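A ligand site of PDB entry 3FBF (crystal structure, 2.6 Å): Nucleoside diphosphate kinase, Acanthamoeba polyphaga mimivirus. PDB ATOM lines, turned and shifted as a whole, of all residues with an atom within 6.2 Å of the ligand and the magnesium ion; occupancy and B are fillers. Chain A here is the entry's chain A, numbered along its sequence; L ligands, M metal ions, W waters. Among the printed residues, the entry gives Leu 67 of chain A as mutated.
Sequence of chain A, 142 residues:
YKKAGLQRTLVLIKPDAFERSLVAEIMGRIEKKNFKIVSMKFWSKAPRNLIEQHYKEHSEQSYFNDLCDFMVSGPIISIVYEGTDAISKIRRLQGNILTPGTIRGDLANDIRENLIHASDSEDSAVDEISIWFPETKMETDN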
ATOM      1  N   LYS A  14      14.246   5.432  -1.820  1.00  0.00           N
ATOM      2  CA  LYS A  14      15.103   6.103  -0.838  1.00  0.00           C
ATOM      3  C   LYS A  14      15.063   5.419   0.533  1.00  0.00           C
ATOM      4  O   LYS A  14      14.219   4.556   0.774  1.00  0.00           O
ATOM      5  CB  LYS A  14      14.727   7.581  -0.755  1.00  0.00           C
ATOM      6  CG  LYS A  14      14.601   8.211  -2.146  1.00  0.00           C
ATOM      7  CD  LYS A  14      14.311   9.691  -2.086  1.00  0.00           C
ATOM      8  CE  LYS A  14      14.505  10.362  -3.439  1.00  0.00           C
ATOM      9  NZ  LYS A  14      14.263  11.820  -3.343  1.00  0.00           N
ATOM     10  N   TYR A  55      22.808  13.642  -8.040  1.00  0.00           N
ATOM     11  CA  TYR A  55      22.239  14.936  -7.695  1.00  0.00           C
ATOM     12  C   TYR A  55      23.159  16.105  -8.034  1.00  0.00           C
ATOM     13  O   TYR A  55      23.078  17.157  -7.398  1.00  0.00           O
ATOM     14  CB  TYR A  55      21.866  14.987  -6.211  1.00  0.00           C
ATOM     15  CG  TYR A  55      20.552  14.296  -5.885  1.00  0.00           C
ATOM     16  CD1 TYR A  55      20.502  13.215  -5.010  1.00  0.00           C
ATOM     17  CD2 TYR A  55      19.359  14.738  -6.448  1.00  0.00           C
ATOM     18  CE1 TYR A  55      19.309  12.579  -4.710  1.00  0.00           C
ATOM     19  CE2 TYR A  55      18.156  14.108  -6.156  1.00  0.00           C
ATOM     20  CZ  TYR A  55      18.133  13.035  -5.285  1.00  0.00           C
ATOM     21  OH  TYR A  55      16.938  12.429  -4.997  1.00  0.00           O
ATOM     22  N   HIS A  58      22.187  19.695  -8.454  1.00  0.00           N
ATOM     23  CA  HIS A  58      21.753  20.348  -7.220  1.00  0.00           C
ATOM     24  C   HIS A  58      22.929  20.726  -6.327  1.00  0.00           C
ATOM     25  O   HIS A  58      22.736  21.107  -5.163  1.00  0.00           O
ATOM     26  CB  HIS A  58      20.808  19.456  -6.412  1.00  0.00           C
ATOM     27  CG  HIS A  58      19.639  18.938  -7.176  1.00  0.00           C
ATOM     28  ND1 HIS A  58      18.368  19.479  -7.051  1.00  0.00           N
ATOM     29  CD2 HIS A  58      19.508  17.896  -8.040  1.00  0.00           C
ATOM     30  CE1 HIS A  58      17.522  18.819  -7.820  1.00  0.00           C
ATOM     31  NE2 HIS A  58      18.199  17.850  -8.428  1.00  0.00           N
ATOM     32  N   TYR A  63      20.141  22.794   0.377  1.00  0.00           N
ATOM     33  CA  TYR A  63      19.742  21.442   0.823  1.00  0.00           C
ATOM     34  C   TYR A  63      20.703  20.341   0.384  1.00  0.00           C
ATOM     35  O   TYR A  63      20.559  19.205   0.824  1.00  0.00           O
ATOM     36  CB  TYR A  63      18.301  21.103   0.363  1.00  0.00           C
ATOM     37  CG  TYR A  63      18.089  21.143  -1.134  1.00  0.00           C
ATOM     38  CD1 TYR A  63      18.552  20.122  -1.952  1.00  0.00           C
ATOM     39  CD2 TYR A  63      17.437  22.212  -1.730  1.00  0.00           C
ATOM     40  CE1 TYR A  63      18.373  20.158  -3.322  1.00  0.00           C
ATOM     41  CE2 TYR A  63      17.245  22.266  -3.095  1.00  0.00           C
ATOM     42  CZ  TYR A  63      17.710  21.228  -3.889  1.00  0.00           C
ATOM     43  OH  TYR A  63      17.537  21.267  -5.253  1.00  0.00           O
ATOM     44  N   ASP A  66      22.542  17.961   3.266  1.00  0.00           N
ATOM     45  CA  ASP A  66      21.551  17.192   4.000  1.00  0.00           C
ATOM     46  C   ASP A  66      20.969  16.119   3.087  1.00  0.00           C
ATOM     47  O   ASP A  66      20.701  14.995   3.507  1.00  0.00           O
ATOM     48  CB  ASP A  66      20.423  18.101   4.492  1.00  0.00           C
ATOM     49  CG  ASP A  66      20.931  19.186   5.438  1.00  0.00           C
ATOM     50  OD1 ASP A  66      21.771  18.866   6.300  1.00  0.00           O
ATOM     51  OD2 ASP A  66      20.474  20.356   5.297  1.00  0.00           O
ATOM     52  N   LEU A  67      20.778  16.471   1.818  1.00  0.00           N
ATOM     53  CA  LEU A  67      20.240  15.551   0.841  1.00  0.00           C
ATOM     54  C   LEU A  67      21.120  14.318   0.783  1.00  0.00           C
ATOM     55  O   LEU A  67      20.663  13.194   1.018  1.00  0.00           O
ATOM     56  CB  LEU A  67      20.158  16.217  -0.538  1.00  0.00           C
ATOM     57  CG  LEU A  67      19.623  15.303  -1.638  1.00  0.00           C
ATOM     58  CD1 LEU A  67      18.302  14.673  -1.235  1.00  0.00           C
ATOM     59  CD2 LEU A  67      19.489  16.046  -2.961  1.00  0.00           C
ATOM     60  N   ARG A  91       6.997   9.444 -13.513  1.00  0.00           N
ATOM     61  CA  ARG A  91       7.194  10.741 -12.876  1.00  0.00           C
ATOM     62  C   ARG A  91       5.890  11.265 -12.322  1.00  0.00           C
ATOM     63  O   ARG A  91       5.834  11.786 -11.214  1.00  0.00           O
ATOM     64  CB  ARG A  91       7.752  11.750 -13.884  1.00  0.00           C
ATOM     65  CG  ARG A  91       8.977  12.478 -13.411  1.00  0.00           C
ATOM     66  CD  ARG A  91       8.676  13.666 -12.511  1.00  0.00           C
ATOM     67  NE  ARG A  91       9.795  13.931 -11.624  1.00  0.00           N
ATOM     68  CZ  ARG A  91      10.134  15.142 -11.165  1.00  0.00           C
ATOM     69  NH1 ARG A  91       9.449  16.219 -11.544  1.00  0.00           N
ATOM     70  NH2 ARG A  91      11.172  15.266 -10.355  1.00  0.00           N
ATOM     71  N   GLN A  94       5.094   9.261  -9.278  1.00  0.00           N
ATOM     72  CA  GLN A  94       5.855   9.725  -8.125  1.00  0.00           C
ATOM     73  C   GLN A  94       5.147  10.901  -7.469  1.00  0.00           C
ATOM     74  O   GLN A  94       4.986  10.940  -6.253  1.00  0.00           O
ATOM     75  CB  GLN A  94       7.265  10.148  -8.546  1.00  0.00           C
ATOM     76  CG  GLN A  94       7.961  11.065  -7.561  1.00  0.00           C
ATOM     77  CD  GLN A  94       9.135  11.822  -8.180  1.00  0.00           C
ATOM     78  OE1 GLN A  94      10.187  11.246  -8.452  1.00  0.00           O
ATOM     79  NE2 GLN A  94       8.957  13.120  -8.394  1.00  0.00           N
ATOM     80  N   GLY A  95       4.722  11.854  -8.282  1.00  0.00           N
ATOM     81  CA  GLY A  95       3.966  13.001  -7.818  1.00  0.00           C
ATOM     82  C   GLY A  95       4.735  13.845  -6.834  1.00  0.00           C
ATOM     83  O   GLY A  95       5.964  13.953  -6.908  1.00  0.00           O
ATOM     84  N   ARG A 104       4.209   9.944  -3.531  1.00  0.00           N
ATOM     85  CA  ARG A 104       4.545  10.932  -2.526  1.00  0.00           C
ATOM     86  C   ARG A 104       3.296  11.558  -1.892  1.00  0.00           C
ATOM     87  O   ARG A 104       3.266  11.804  -0.693  1.00  0.00           O
ATOM     88  CB  ARG A 104       5.442  12.018  -3.109  1.00  0.00           C
ATOM     89  CG  ARG A 104       6.855  11.559  -3.432  1.00  0.00           C
ATOM     90  CD  ARG A 104       7.707  12.749  -3.848  1.00  0.00           C
ATOM     91  NE  ARG A 104       8.943  12.358  -4.504  1.00  0.00           N
ATOM     92  CZ  ARG A 104       9.820  13.217  -5.013  1.00  0.00           C
ATOM     93  NH1 ARG A 104       9.589  14.527  -4.937  1.00  0.00           N
ATOM     94  NH2 ARG A 104      10.933  12.777  -5.593  1.00  0.00           N
ATOM     95  N   ILE A 111       9.937  17.433   2.660  1.00  0.00           N
ATOM     96  CA  ILE A 111      10.565  17.950   1.436  1.00  0.00           C
ATOM     97  C   ILE A 111      11.828  17.195   1.067  1.00  0.00           C
ATOM     98  O   ILE A 111      12.281  17.256  -0.075  1.00  0.00           O
ATOM     99  CB  ILE A 111      10.966  19.432   1.566  1.00  0.00           C
ATOM    100  CG1 ILE A 111      11.223  19.761   3.036  1.00  0.00           C
ATOM    101  CG2 ILE A 111       9.898  20.338   0.946  1.00  0.00           C
ATOM    102  CD1 ILE A 111      12.507  20.526   3.254  1.00  0.00           C
ATOM    103  N   ARG A 112      12.402  16.489   2.036  1.00  0.00           N
ATOM    104  CA  ARG A 112      13.625  15.728   1.799  1.00  0.00           C
ATOM    105  C   ARG A 112      13.357  14.216   1.771  1.00  0.00           C
ATOM    106  O   ARG A 112      13.668  13.537   0.782  1.00  0.00           O
ATOM    107  CB  ARG A 112      14.664  16.046   2.873  1.00  0.00           C
ATOM    108  CG  ARG A 112      16.086  15.617   2.523  1.00  0.00           C
ATOM    109  CD  ARG A 112      17.015  15.869   3.681  1.00  0.00           C
ATOM    110  NE  ARG A 112      16.841  14.857   4.721  1.00  0.00           N
ATOM    111  CZ  ARG A 112      16.972  15.081   6.018  1.00  0.00           C
ATOM    112  NH1 ARG A 112      17.286  16.293   6.457  1.00  0.00           N
ATOM    113  NH2 ARG A 112      16.792  14.087   6.890  1.00  0.00           N
ATOM    114  N   GLU A 113      12.791  13.700   2.852  1.00  0.00           N
ATOM    115  CA  GLU A 113      12.445  12.286   2.951  1.00  0.00           C
ATOM    116  C   GLU A 113      11.140  12.035   2.199  1.00  0.00           C
ATOM    117  O   GLU A 113      10.051  12.131   2.760  1.00  0.00           O
ATOM    118  CB  GLU A 113      12.316  11.871   4.409  1.00  0.00           C
ATOM    119  CG  GLU A 113      13.350  12.534   5.312  1.00  0.00           C
ATOM    120  CD  GLU A 113      13.649  11.726   6.551  1.00  0.00           C
ATOM    121  OE1 GLU A 113      12.800  10.891   6.932  1.00  0.00           O
ATOM    122  OE2 GLU A 113      14.725  11.930   7.158  1.00  0.00           O
ATOM    123  N   ASN A 114      11.263  11.711   0.911  1.00  0.00           N
ATOM    124  CA  ASN A 114      10.074  11.559   0.083  1.00  0.00           C
ATOM    125  C   ASN A 114      10.019  10.245  -0.701  1.00  0.00           C
ATOM    126  O   ASN A 114       9.374  10.169  -1.746  1.00  0.00           O
ATOM    127  CB  ASN A 114       9.881  12.770  -0.828  1.00  0.00           C
ATOM    128  CG  ASN A 114      11.113  13.086  -1.640  1.00  0.00           C
ATOM    129  OD1 ASN A 114      12.012  12.259  -1.780  1.00  0.00           O
ATOM    130  ND2 ASN A 114      11.169  14.299  -2.178  1.00  0.00           N
ATOM    131  N   ILE A 116      10.968   8.294  -2.971  1.00  0.00           N
ATOM    132  CA  ILE A 116      11.263   7.875  -4.339  1.00  0.00           C
ATOM    133  C   ILE A 116      11.827   8.963  -5.246  1.00  0.00           C
ATOM    134  O   ILE A 116      11.443  10.131  -5.177  1.00  0.00           O
ATOM    135  CB  ILE A 116       9.997   7.297  -5.020  1.00  0.00           C
ATOM    136  CG1 ILE A 116      10.263   7.003  -6.498  1.00  0.00           C
ATOM    137  CG2 ILE A 116       8.802   8.237  -4.844  1.00  0.00           C
ATOM    138  CD1 ILE A 116       9.165   6.234  -7.170  1.00  0.00           C
ATOM    139  N   HIS A 117      12.759   8.557  -6.103  1.00  0.00           N
ATOM    140  CA  HIS A 117      13.191   9.387  -7.215  1.00  0.00           C
ATOM    141  C   HIS A 117      12.884   8.753  -8.567  1.00  0.00           C
ATOM    142  O   HIS A 117      13.127   7.564  -8.786  1.00  0.00           O
ATOM    143  CB  HIS A 117      14.686   9.657  -7.166  1.00  0.00           C
ATOM    144  CG  HIS A 117      15.222  10.245  -8.429  1.00  0.00           C
ATOM    145  ND1 HIS A 117      15.478  11.594  -8.567  1.00  0.00           N
ATOM    146  CD2 HIS A 117      15.495   9.674  -9.626  1.00  0.00           C
ATOM    147  CE1 HIS A 117      15.906  11.826  -9.799  1.00  0.00           C
ATOM    148  NE2 HIS A 117      15.929  10.678 -10.465  1.00  0.00           N
ATOM    149  N   ALA A 118      12.374   9.571  -9.474  1.00  0.00           N
ATOM    150  CA  ALA A 118      12.176   9.157 -10.856  1.00  0.00           C
ATOM    151  C   ALA A 118      12.787  10.190 -11.809  1.00  0.00           C
ATOM    152  O   ALA A 118      12.683  11.393 -11.569  1.00  0.00           O
ATOM    153  CB  ALA A 118      10.696   8.953 -11.155  1.00  0.00           C
ATOM    154  N   ASP A 120      13.259  12.756 -14.713  1.00  0.00           N
ATOM    155  CA  ASP A 120      12.248  13.704 -15.144  1.00  0.00           C
ATOM    156  C   ASP A 120      12.334  14.083 -16.614  1.00  0.00           C
ATOM    157  O   ASP A 120      11.532  14.878 -17.102  1.00  0.00           O
ATOM    158  CB  ASP A 120      12.274  14.957 -14.276  1.00  0.00           C
ATOM    159  CG  ASP A 120      13.541  15.767 -14.473  1.00  0.00           C
ATOM    160  OD1 ASP A 120      14.395  15.344 -15.278  1.00  0.00           O
ATOM    161  OD2 ASP A 120      13.673  16.834 -13.822  1.00  0.00           O
HETATM  162  P1  LIG L   1      13.584  18.435  -6.287  1.00  0.00           P
HETATM  163  O1  LIG L   1      14.135  18.272  -7.682  1.00  0.00           O
HETATM  164  O2  LIG L   1      13.028  19.760  -5.826  1.00  0.00           O
HETATM  165  O3  LIG L   1      12.448  17.301  -5.984  1.00  0.00           O
HETATM  166  P2  LIG L   1      12.223  15.981  -6.888  1.00  0.00           P
HETATM  167  O4  LIG L   1      12.899  14.842  -6.154  1.00  0.00           O
HETATM  168  O5  LIG L   1      12.856  16.272  -8.234  1.00  0.00           O
HETATM  169  O6  LIG L   1      10.722  15.910  -6.933  1.00  0.00           O
HETATM  170  O7  LIG L   1      14.702  17.996  -5.221  1.00  0.00           O
HETATM  171  C1  LIG L   1      15.502  16.851  -5.459  1.00  0.00           C
HETATM  172  C2  LIG L   1      15.636  16.176  -4.105  1.00  0.00           C
HETATM  173  O8  LIG L   1      16.301  17.082  -3.209  1.00  0.00           O
HETATM  174  C3  LIG L   1      14.265  15.904  -3.510  1.00  0.00           C
HETATM  175  O9  LIG L   1      13.865  14.564  -3.764  1.00  0.00           O
HETATM  176  C4  LIG L   1      14.438  16.145  -2.026  1.00  0.00           C
HETATM  177  C5  LIG L   1      15.661  17.065  -1.928  1.00  0.00           C
HETATM  178  N1  LIG L   1      15.237  18.405  -1.502  1.00  0.00           N
HETATM  179  C6  LIG L   1      15.479  18.755  -0.156  1.00  0.00           C
HETATM  180  O10 LIG L   1      16.030  17.929   0.604  1.00  0.00           O
HETATM  181  N2  LIG L   1      15.139  19.958   0.320  1.00  0.00           N
HETATM  182  C7  LIG L   1      14.554  20.866  -0.458  1.00  0.00           C
HETATM  183  O11 LIG L   1      14.243  21.992   0.007  1.00  0.00           O
HETATM  184  C8  LIG L   1      14.290  20.530  -1.883  1.00  0.00           C
HETATM  185  C9  LIG L   1      13.635  21.548  -2.780  1.00  0.00           C
HETATM  186  C10 LIG L   1      14.669  19.277  -2.348  1.00  0.00           C
HETATM  187 MG    MG M   1      13.702  17.717 -10.128  1.00  0.00          MG
HETATM  188  O   HOH W   1      15.418  15.753  -8.978  1.00  0.00           O
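A nitrogen (N1) of the ligand lies close to the backbone carbonyl oxygen (O) of Ile 111. Residues that only touch the ligand: Arg 112 (3.0 Å), Leu 67 (3.4 Å), Tyr 63 (3.4 Å), His 58 (3.4 Å), Gln 94 (3.6 Å) and Tyr 55 (3.9 Å). Hydrophobic or aromatic side chains within 4 Å of the ligand: Tyr 55, His 58, Tyr 63, Leu 67 and Ile 111.
The magnesium ion is bound by O5 of the ligand (2.5 Å) and O1 of the ligand (2.5 Å).
The side-chain amide nitrogen (ND2) of Asn 114 sits at hydrogen-bond distance from an oxygen (O9) of the ligand (3.1 Å). The side-chain amino group (NZ) of Lys 14 is in hydrogen-bond range of an oxygen (O9) of the ligand. O6 of the ligand is in salt-bridge range of NH2 of Arg 91 (3.5 Å). The guanidinium group (NH1) of Arg 104 lies within salt-bridge range of an oxygen (O6) of the ligand (2.7 Å).
A ring nitrogen (ND1) of His 58 lies within hydrogen-bond range of the side-chain hydroxyl (OH) of Tyr 63 (2.7 Å). NH2 of Arg 112 is in salt-bridge range of OE2 of Glu 113 (3.0 Å). O of Ile 116 is in hydrogen-bond range of NH2 of Arg 104. The side-chain amino group (NZ) of Lys 14 lies within hydrogen-bond range of the side-chain amide oxygen (OD1) of Asn 114 (2.8 Å). NZ of Lys 14 lies within hydrogen-bond range of OH of Tyr 55, 3.2 Å away. The backbone carbonyl oxygen (O) of Arg 112 sits close to the side-chain amide oxygen (OD1) of Asn 114, at 3.3 Å. ND2 of Asn 114 lies close to NH1 of Arg 104 (3.2 Å). NE of Arg 91 sits close to NE2 of Gln 94 (3.4 Å).
Residues that only touch the magnesium ion: Arg 91 (3.5 Å) and Asp 120 (3.8 Å). Of the 18 residues printed, 2 come within 4 Å of the magnesium ion. Along chain A the residues within 4 Å of the magnesium ion span positions 91 to 120. The nearest printed residue that does not touch the magnesium ion is His 58 (4.6 Å).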
